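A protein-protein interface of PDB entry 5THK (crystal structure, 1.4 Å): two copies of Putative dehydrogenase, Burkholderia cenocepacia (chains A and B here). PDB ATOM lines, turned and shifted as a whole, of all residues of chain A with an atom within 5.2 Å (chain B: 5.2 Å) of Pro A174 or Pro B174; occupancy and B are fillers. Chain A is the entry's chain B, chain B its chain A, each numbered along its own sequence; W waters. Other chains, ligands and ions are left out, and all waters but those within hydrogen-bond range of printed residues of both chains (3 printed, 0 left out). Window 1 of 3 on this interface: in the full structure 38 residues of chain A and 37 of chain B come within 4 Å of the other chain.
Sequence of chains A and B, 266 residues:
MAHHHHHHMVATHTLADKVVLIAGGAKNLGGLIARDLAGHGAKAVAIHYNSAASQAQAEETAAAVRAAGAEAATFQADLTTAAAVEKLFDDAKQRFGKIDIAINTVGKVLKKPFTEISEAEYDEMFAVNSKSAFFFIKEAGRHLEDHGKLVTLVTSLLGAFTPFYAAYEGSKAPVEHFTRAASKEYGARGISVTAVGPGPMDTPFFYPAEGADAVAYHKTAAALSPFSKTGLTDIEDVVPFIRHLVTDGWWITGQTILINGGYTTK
Among the printed residues, pairs that only touch across the chains: Phe A126 with Ser B130 (3.3 Å), Phe A126 with Pro B174 (3.9 Å), Phe A126 with Phe B178 (3.6 Å), Ser A130 with Phe B126 (3.4 Å), Gly A170 with Pro B174 (3.2 Å), Gly A170 with Phe B178 (3.9 Å), Ala A173 with Ala B173 (3.995 Å), Ala A173 with His B177 (3.4 Å), Pro A174 with Phe B126 (3.9 Å), Pro A174 with Gly B170 (3.2 Å), Pro A174 with Pro B174 (3.6 Å), His A177 with Ala B173 (3.4 Å), Phe A178 with Phe B126 (3.6 Å) and Phe A178 with Gly B170 (3.9 Å).
Pro A174 touches just these residues of chain B: Phe B126 (3.9 Å), Gly B170 (3.2 Å) and Pro B174 (3.6 Å). Of the printed residues of chain A, Phe B178 touches Phe A126 and Gly A170. Of the printed residues of chain B, Phe A126 touches Ser B130, Pro B174 and Phe B178. Of the printed residues of chain B, His A177 touches Ala B173 (3.4 Å). The nearest residue of chain B that does not touch Pro A174 is Ala B173 (4.4 Å).
Hydrophobic or aromatic side chains of chain B that line the printed part of chain A: Phe B126, Ala B173, Pro B174, His B177 and Phe B178. Hydrophobic or aromatic side chains of chain A within 4 Å of the printed part of chain B: Phe A126, Ala A173, Pro A174, His A177 and Phe A178. Among the printed residues, 14 pairs touch across the chains.
Phe A126 touches Pro B174, and with the chains exchanged Pro A174 touches Phe B126. Phe A126 touches Phe B178, and with the chains exchanged Phe A178 touches Phe B126. Gly A170 touches Pro B174, and with the chains exchanged Pro A174 touches Gly B170. Ala A173 touches its own counterpart, Ala B173. 12 positions are printed for both chains. Of the 14 pairs that touch across the chains among the printed residues, 14 have their exchanged pair printed and touching as well.
Water W3 lies within hydrogen-bond range of a ring nitrogen (NE2) of His B177 (2.9 Å) and the side-chain carboxylate (OE1) of Glu A176 (3.1 Å). Water W2 bridges NE2 of His A177 (3.0 Å) and OE1 of Glu B176 (3.2 Å). Water W1 lies within hydrogen-bond range of OE1 of Glu A176, O of Ala A173, NE2 of His A177 and NE2 of His B177.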
ATOM      1  N   PHE A 126      29.847 -15.592   8.822  1.00  0.00           N
ATOM      2  CA  PHE A 126      30.284 -14.555   7.894  1.00  0.00           C
ATOM      3  C   PHE A 126      30.991 -15.107   6.662  1.00  0.00           C
ATOM      4  O   PHE A 126      30.842 -14.531   5.573  1.00  0.00           O
ATOM      5  CB  PHE A 126      31.056 -13.461   8.626  1.00  0.00           C
ATOM      6  CG  PHE A 126      30.153 -12.423   9.197  1.00  0.00           C
ATOM      7  CD1 PHE A 126      29.425 -12.661  10.363  1.00  0.00           C
ATOM      8  CD2 PHE A 126      29.956 -11.234   8.524  1.00  0.00           C
ATOM      9  CE1 PHE A 126      28.548 -11.702  10.861  1.00  0.00           C
ATOM     10  CE2 PHE A 126      29.079 -10.284   9.016  1.00  0.00           C
ATOM     11  CZ  PHE A 126      28.378 -10.521  10.188  1.00  0.00           C
ATOM     12  N   SER A 130      28.434 -13.860   3.960  1.00  0.00           N
ATOM     13  CA  SER A 130      28.992 -12.621   3.439  1.00  0.00           C
ATOM     14  C   SER A 130      30.146 -12.856   2.474  1.00  0.00           C
ATOM     15  O   SER A 130      30.106 -12.376   1.336  1.00  0.00           O
ATOM     16  CB  SER A 130      29.411 -11.683   4.582  1.00  0.00           C
ATOM     17  OG  SER A 130      29.947 -10.482   4.049  1.00  0.00           O
ATOM     18  N   GLY A 170      22.820 -10.025  10.358  1.00  0.00           N
ATOM     19  CA  GLY A 170      24.009  -9.204  10.180  1.00  0.00           C
ATOM     20  C   GLY A 170      24.944  -9.680   9.084  1.00  0.00           C
ATOM     21  O   GLY A 170      25.647  -8.864   8.475  1.00  0.00           O
ATOM     22  N   SER A 171      25.003 -10.995   8.833  1.00  0.00           N
ATOM     23  CA  SER A 171      25.885 -11.510   7.786  1.00  0.00           C
ATOM     24  C   SER A 171      25.247 -11.537   6.404  1.00  0.00           C
ATOM     25  O   SER A 171      25.970 -11.672   5.407  1.00  0.00           O
ATOM     26  CB  SER A 171      26.475 -12.881   8.151  1.00  0.00           C
ATOM     27  OG  SER A 171      25.474 -13.887   8.254  1.00  0.00           O
ATOM     28  N   LYS A 172      23.920 -11.425   6.311  1.00  0.00           N
ATOM     29  CA  LYS A 172      23.273 -11.207   5.025  1.00  0.00           C
ATOM     30  C   LYS A 172      23.207  -9.734   4.650  1.00  0.00           C
ATOM     31  O   LYS A 172      23.167  -9.417   3.460  1.00  0.00           O
ATOM     32  CB  LYS A 172      21.850 -11.787   5.024  1.00  0.00           C
ATOM     33  CG  LYS A 172      21.767 -13.317   5.050  1.00  0.00           C
ATOM     34  CD  LYS A 172      22.288 -13.943   3.768  1.00  0.00           C
ATOM     35  CE  LYS A 172      21.774 -15.371   3.612  1.00  0.00           C
ATOM     36  NZ  LYS A 172      22.186 -15.942   2.301  1.00  0.00           N
ATOM     37  N   ALA A 173      23.241  -8.832   5.632  1.00  0.00           N
ATOM     38  CA  ALA A 173      23.182  -7.398   5.348  1.00  0.00           C
ATOM     39  C   ALA A 173      24.229  -6.900   4.357  1.00  0.00           C
ATOM     40  O   ALA A 173      23.895  -6.011   3.554  1.00  0.00           O
ATOM     41  CB  ALA A 173      23.254  -6.603   6.660  1.00  0.00           C
ATOM     42  N   PRO A 174      25.479  -7.381   4.362  1.00  0.00           N
ATOM     43  CA  PRO A 174      26.443  -6.869   3.373  1.00  0.00           C
ATOM     44  C   PRO A 174      25.983  -7.068   1.942  1.00  0.00           C
ATOM     45  O   PRO A 174      26.303  -6.240   1.081  1.00  0.00           O
ATOM     46  CB  PRO A 174      27.714  -7.676   3.674  1.00  0.00           C
ATOM     47  CG  PRO A 174      27.584  -8.010   5.124  1.00  0.00           C
ATOM     48  CD  PRO A 174      26.128  -8.325   5.291  1.00  0.00           C
ATOM     49  N   VAL A 175      25.230  -8.139   1.675  1.00  0.00           N
ATOM     50  CA  VAL A 175      24.811  -8.461   0.312  1.00  0.00           C
ATOM     51  C   VAL A 175      23.962  -7.343  -0.293  1.00  0.00           C
ATOM     52  O   VAL A 175      24.046  -7.063  -1.498  1.00  0.00           O
ATOM     53  CB  VAL A 175      24.088  -9.820   0.292  1.00  0.00           C
ATOM     54  CG1 VAL A 175      23.555 -10.103  -1.106  1.00  0.00           C
ATOM     55  CG2 VAL A 175      25.018 -10.929   0.753  1.00  0.00           C
ATOM     56  N   GLU A 176      23.117  -6.701   0.518  1.00  0.00           N
ATOM     57  CA  GLU A 176      22.340  -5.583  -0.003  1.00  0.00           C
ATOM     58  C   GLU A 176      23.259  -4.506  -0.553  1.00  0.00           C
ATOM     59  O   GLU A 176      23.004  -3.939  -1.621  1.00  0.00           O
ATOM     60  CB  GLU A 176      21.450  -4.998   1.097  1.00  0.00           C
ATOM     61  CG  GLU A 176      20.804  -3.691   0.677  1.00  0.00           C
ATOM     62  CD  GLU A 176      19.715  -3.231   1.611  1.00  0.00           C
ATOM     63  OE1 GLU A 176      19.576  -3.814   2.706  1.00  0.00           O
ATOM     64  OE2 GLU A 176      19.000  -2.270   1.240  1.00  0.00           O
ATOM     65  N   HIS A 177      24.350  -4.226   0.160  1.00  0.00           N
ATOM     66  CA  HIS A 177      25.260  -3.168  -0.254  1.00  0.00           C
ATOM     67  C   HIS A 177      26.213  -3.610  -1.355  1.00  0.00           C
ATOM     68  O   HIS A 177      26.538  -2.807  -2.238  1.00  0.00           O
ATOM     69  CB  HIS A 177      25.941  -2.590   0.984  1.00  0.00           C
ATOM     70  CG  HIS A 177      24.956  -1.959   1.911  1.00  0.00           C
ATOM     71  ND1 HIS A 177      24.614  -0.629   1.827  1.00  0.00           N
ATOM     72  CD2 HIS A 177      24.166  -2.496   2.871  1.00  0.00           C
ATOM     73  CE1 HIS A 177      23.677  -0.363   2.723  1.00  0.00           C
ATOM     74  NE2 HIS A 177      23.388  -1.479   3.369  1.00  0.00           N
ATOM     75  N   PHE A 178      26.652  -4.872  -1.343  1.00  0.00           N
ATOM     76  CA  PHE A 178      27.363  -5.397  -2.506  1.00  0.00           C
ATOM     77  C   PHE A 178      26.513  -5.259  -3.766  1.00  0.00           C
ATOM     78  O   PHE A 178      27.030  -4.954  -4.849  1.00  0.00           O
ATOM     79  CB  PHE A 178      27.667  -6.886  -2.337  1.00  0.00           C
ATOM     80  CG  PHE A 178      28.493  -7.261  -1.128  1.00  0.00           C
ATOM     81  CD1 PHE A 178      29.301  -6.353  -0.458  1.00  0.00           C
ATOM     82  CD2 PHE A 178      28.465  -8.574  -0.691  1.00  0.00           C
ATOM     83  CE1 PHE A 178      30.050  -6.766   0.655  1.00  0.00           C
ATOM     84  CE2 PHE A 178      29.188  -8.983   0.415  1.00  0.00           C
ATOM     85  CZ  PHE A 178      29.999  -8.077   1.086  1.00  0.00           C
ATOM     86  N   THR A 179      25.212  -5.526  -3.639  1.00  0.00           N
ATOM     87  CA  THR A 179      24.283  -5.457  -4.763  1.00  0.00           C
ATOM     88  C   THR A 179      24.156  -4.032  -5.298  1.00  0.00           C
ATOM     89  O   THR A 179      24.083  -3.830  -6.518  1.00  0.00           O
ATOM     90  CB  THR A 179      22.944  -6.061  -4.313  1.00  0.00           C
ATOM     91  OG1 THR A 179      23.122  -7.473  -4.094  1.00  0.00           O
ATOM     92  CG2 THR A 179      21.824  -5.824  -5.334  1.00  0.00           C
ATOM     93  N   PHE B 126      36.515  -6.739   6.550  1.00  0.00           N
ATOM     94  CA  PHE B 126      35.463  -7.342   7.361  1.00  0.00           C
ATOM     95  C   PHE B 126      35.906  -7.628   8.789  1.00  0.00           C
ATOM     96  O   PHE B 126      35.097  -7.487   9.716  1.00  0.00           O
ATOM     97  CB  PHE B 126      34.839  -8.539   6.648  1.00  0.00           C
ATOM     98  CG  PHE B 126      33.740  -8.126   5.736  1.00  0.00           C
ATOM     99  CD1 PHE B 126      34.030  -7.583   4.488  1.00  0.00           C
ATOM    100  CD2 PHE B 126      32.426  -8.171   6.160  1.00  0.00           C
ATOM    101  CE1 PHE B 126      33.014  -7.141   3.671  1.00  0.00           C
ATOM    102  CE2 PHE B 126      31.421  -7.733   5.342  1.00  0.00           C
ATOM    103  CZ  PHE B 126      31.713  -7.222   4.100  1.00  0.00           C
ATOM    104  N   SER B 130      33.402  -5.213  10.659  1.00  0.00           N
ATOM    105  CA  SER B 130      32.298  -6.070  11.091  1.00  0.00           C
ATOM    106  C   SER B 130      32.647  -6.901  12.318  1.00  0.00           C
ATOM    107  O   SER B 130      31.952  -6.806  13.332  1.00  0.00           O
ATOM    108  CB  SER B 130      31.802  -6.971   9.951  1.00  0.00           C
ATOM    109  OG  SER B 130      30.745  -7.822  10.393  1.00  0.00           O
ATOM    110  N   GLY B 170      29.724  -2.313   2.635  1.00  0.00           N
ATOM    111  CA  GLY B 170      29.271  -3.664   2.925  1.00  0.00           C
ATOM    112  C   GLY B 170      29.733  -4.200   4.268  1.00  0.00           C
ATOM    113  O   GLY B 170      29.030  -5.003   4.889  1.00  0.00           O
ATOM    114  N   SER B 171      30.907  -3.768   4.744  1.00  0.00           N
ATOM    115  CA  SER B 171      31.400  -4.240   6.040  1.00  0.00           C
ATOM    116  C   SER B 171      30.925  -3.405   7.219  1.00  0.00           C
ATOM    117  O   SER B 171      31.014  -3.875   8.361  1.00  0.00           O
ATOM    118  CB  SER B 171      32.925  -4.398   6.056  1.00  0.00           C
ATOM    119  OG  SER B 171      33.599  -3.161   5.891  1.00  0.00           O
ATOM    120  N   LYS B 172      30.407  -2.198   6.977  1.00  0.00           N
ATOM    121  CA  LYS B 172      29.724  -1.438   8.019  1.00  0.00           C
ATOM    122  C   LYS B 172      28.256  -1.821   8.143  1.00  0.00           C
ATOM    123  O   LYS B 172      27.681  -1.701   9.233  1.00  0.00           O
ATOM    124  CB  LYS B 172      29.824   0.072   7.753  1.00  0.00           C
ATOM    125  CG  LYS B 172      31.219   0.690   7.970  1.00  0.00           C
ATOM    126  CD  LYS B 172      31.685   0.572   9.411  1.00  0.00           C
ATOM    127  CE  LYS B 172      32.836   1.536   9.674  1.00  0.00           C
ATOM    128  NZ  LYS B 172      33.293   1.492  11.096  1.00  0.00           N
ATOM    129  N   ALA B 173      27.655  -2.318   7.060  1.00  0.00           N
ATOM    130  CA  ALA B 173      26.243  -2.702   7.088  1.00  0.00           C
ATOM    131  C   ALA B 173      25.869  -3.673   8.204  1.00  0.00           C
ATOM    132  O   ALA B 173      24.780  -3.511   8.786  1.00  0.00           O
ATOM    133  CB  ALA B 173      25.814  -3.260   5.725  1.00  0.00           C
ATOM    134  N   PRO B 174      26.674  -4.676   8.554  1.00  0.00           N
ATOM    135  CA  PRO B 174      26.261  -5.562   9.653  1.00  0.00           C
ATOM    136  C   PRO B 174      26.004  -4.824  10.949  1.00  0.00           C
ATOM    137  O   PRO B 174      25.131  -5.232  11.725  1.00  0.00           O
ATOM    138  CB  PRO B 174      27.447  -6.517   9.782  1.00  0.00           C
ATOM    139  CG  PRO B 174      28.061  -6.544   8.413  1.00  0.00           C
ATOM    140  CD  PRO B 174      27.936  -5.132   7.938  1.00  0.00           C
ATOM    141  N   VAL B 175      26.721  -3.725  11.191  1.00  0.00           N
ATOM    142  CA  VAL B 175      26.597  -3.013  12.463  1.00  0.00           C
ATOM    143  C   VAL B 175      25.177  -2.504  12.680  1.00  0.00           C
ATOM    144  O   VAL B 175      24.673  -2.503  13.813  1.00  0.00           O
ATOM    145  CB  VAL B 175      27.642  -1.884  12.541  1.00  0.00           C
ATOM    146  CG1 VAL B 175      27.438  -1.049  13.802  1.00  0.00           C
ATOM    147  CG2 VAL B 175      29.052  -2.468  12.480  1.00  0.00           C
ATOM    148  N   GLU B 176      24.505  -2.055  11.614  1.00  0.00           N
ATOM    149  CA  GLU B 176      23.124  -1.603  11.772  1.00  0.00           C
ATOM    150  C   GLU B 176      22.252  -2.725  12.316  1.00  0.00           C
ATOM    151  O   GLU B 176      21.396  -2.508  13.186  1.00  0.00           O
ATOM    152  CB  GLU B 176      22.580  -1.103  10.431  1.00  0.00           C
ATOM    153  CG  GLU B 176      21.068  -0.916  10.443  1.00  0.00           C
ATOM    154  CD  GLU B 176      20.541  -0.111   9.274  1.00  0.00           C
ATOM    155  OE1 GLU B 176      21.304   0.128   8.309  1.00  0.00           O
ATOM    156  OE2 GLU B 176      19.357   0.290   9.328  1.00  0.00           O
ATOM    157  N   HIS B 177      22.471  -3.939  11.821  1.00  0.00           N
ATOM    158  CA  HIS B 177      21.664  -5.073  12.239  1.00  0.00           C
ATOM    159  C   HIS B 177      22.115  -5.626  13.588  1.00  0.00           C
ATOM    160  O   HIS B 177      21.270  -6.032  14.396  1.00  0.00           O
ATOM    161  CB  HIS B 177      21.602  -6.101  11.105  1.00  0.00           C
ATOM    162  CG  HIS B 177      20.948  -5.542   9.881  1.00  0.00           C
ATOM    163  ND1 HIS B 177      19.588  -5.609   9.669  1.00  0.00           N
ATOM    164  CD2 HIS B 177      21.452  -4.795   8.870  1.00  0.00           C
ATOM    165  CE1 HIS B 177      19.290  -4.973   8.549  1.00  0.00           C
ATOM    166  NE2 HIS B 177      20.403  -4.466   8.049  1.00  0.00           N
ATOM    167  N   PHE B 178      23.426  -5.616  13.874  1.00  0.00           N
ATOM    168  CA  PHE B 178      23.867  -5.926  15.234  1.00  0.00           C
ATOM    169  C   PHE B 178      23.207  -4.981  16.234  1.00  0.00           C
ATOM    170  O   PHE B 178      22.835  -5.388  17.340  1.00  0.00           O
ATOM    171  CB  PHE B 178      25.382  -5.752  15.385  1.00  0.00           C
ATOM    172  CG  PHE B 178      26.239  -6.591  14.463  1.00  0.00           C
ATOM    173  CD1 PHE B 178      25.772  -7.752  13.846  1.00  0.00           C
ATOM    174  CD2 PHE B 178      27.560  -6.207  14.248  1.00  0.00           C
ATOM    175  CE1 PHE B 178      26.609  -8.489  13.005  1.00  0.00           C
ATOM    176  CE2 PHE B 178      28.398  -6.945  13.418  1.00  0.00           C
ATOM    177  CZ  PHE B 178      27.921  -8.081  12.798  1.00  0.00           C
ATOM    178  N   THR B 179      23.076  -3.704  15.861  1.00  0.00           N
ATOM    179  CA  THR B 179      22.513  -2.695  16.754  1.00  0.00           C
ATOM    180  C   THR B 179      21.026  -2.951  17.010  1.00  0.00           C
ATOM    181  O   THR B 179      20.552  -2.789  18.140  1.00  0.00           O
ATOM    182  CB  THR B 179      22.789  -1.313  16.137  1.00  0.00           C
ATOM    183  OG1 THR B 179      24.208  -1.065  16.159  1.00  0.00           O
ATOM    184  CG2 THR B 179      22.071  -0.197  16.865  1.00  0.00           C
HETATM  185  O   HOH W   1      21.831  -3.928   5.018  1.00  0.00           O
HETATM  186  O   HOH W   2      21.246  -0.730   5.277  1.00  0.00           O
HETATM  187  O   HOH W   3      19.461  -3.029   5.655  1.00  0.00           O
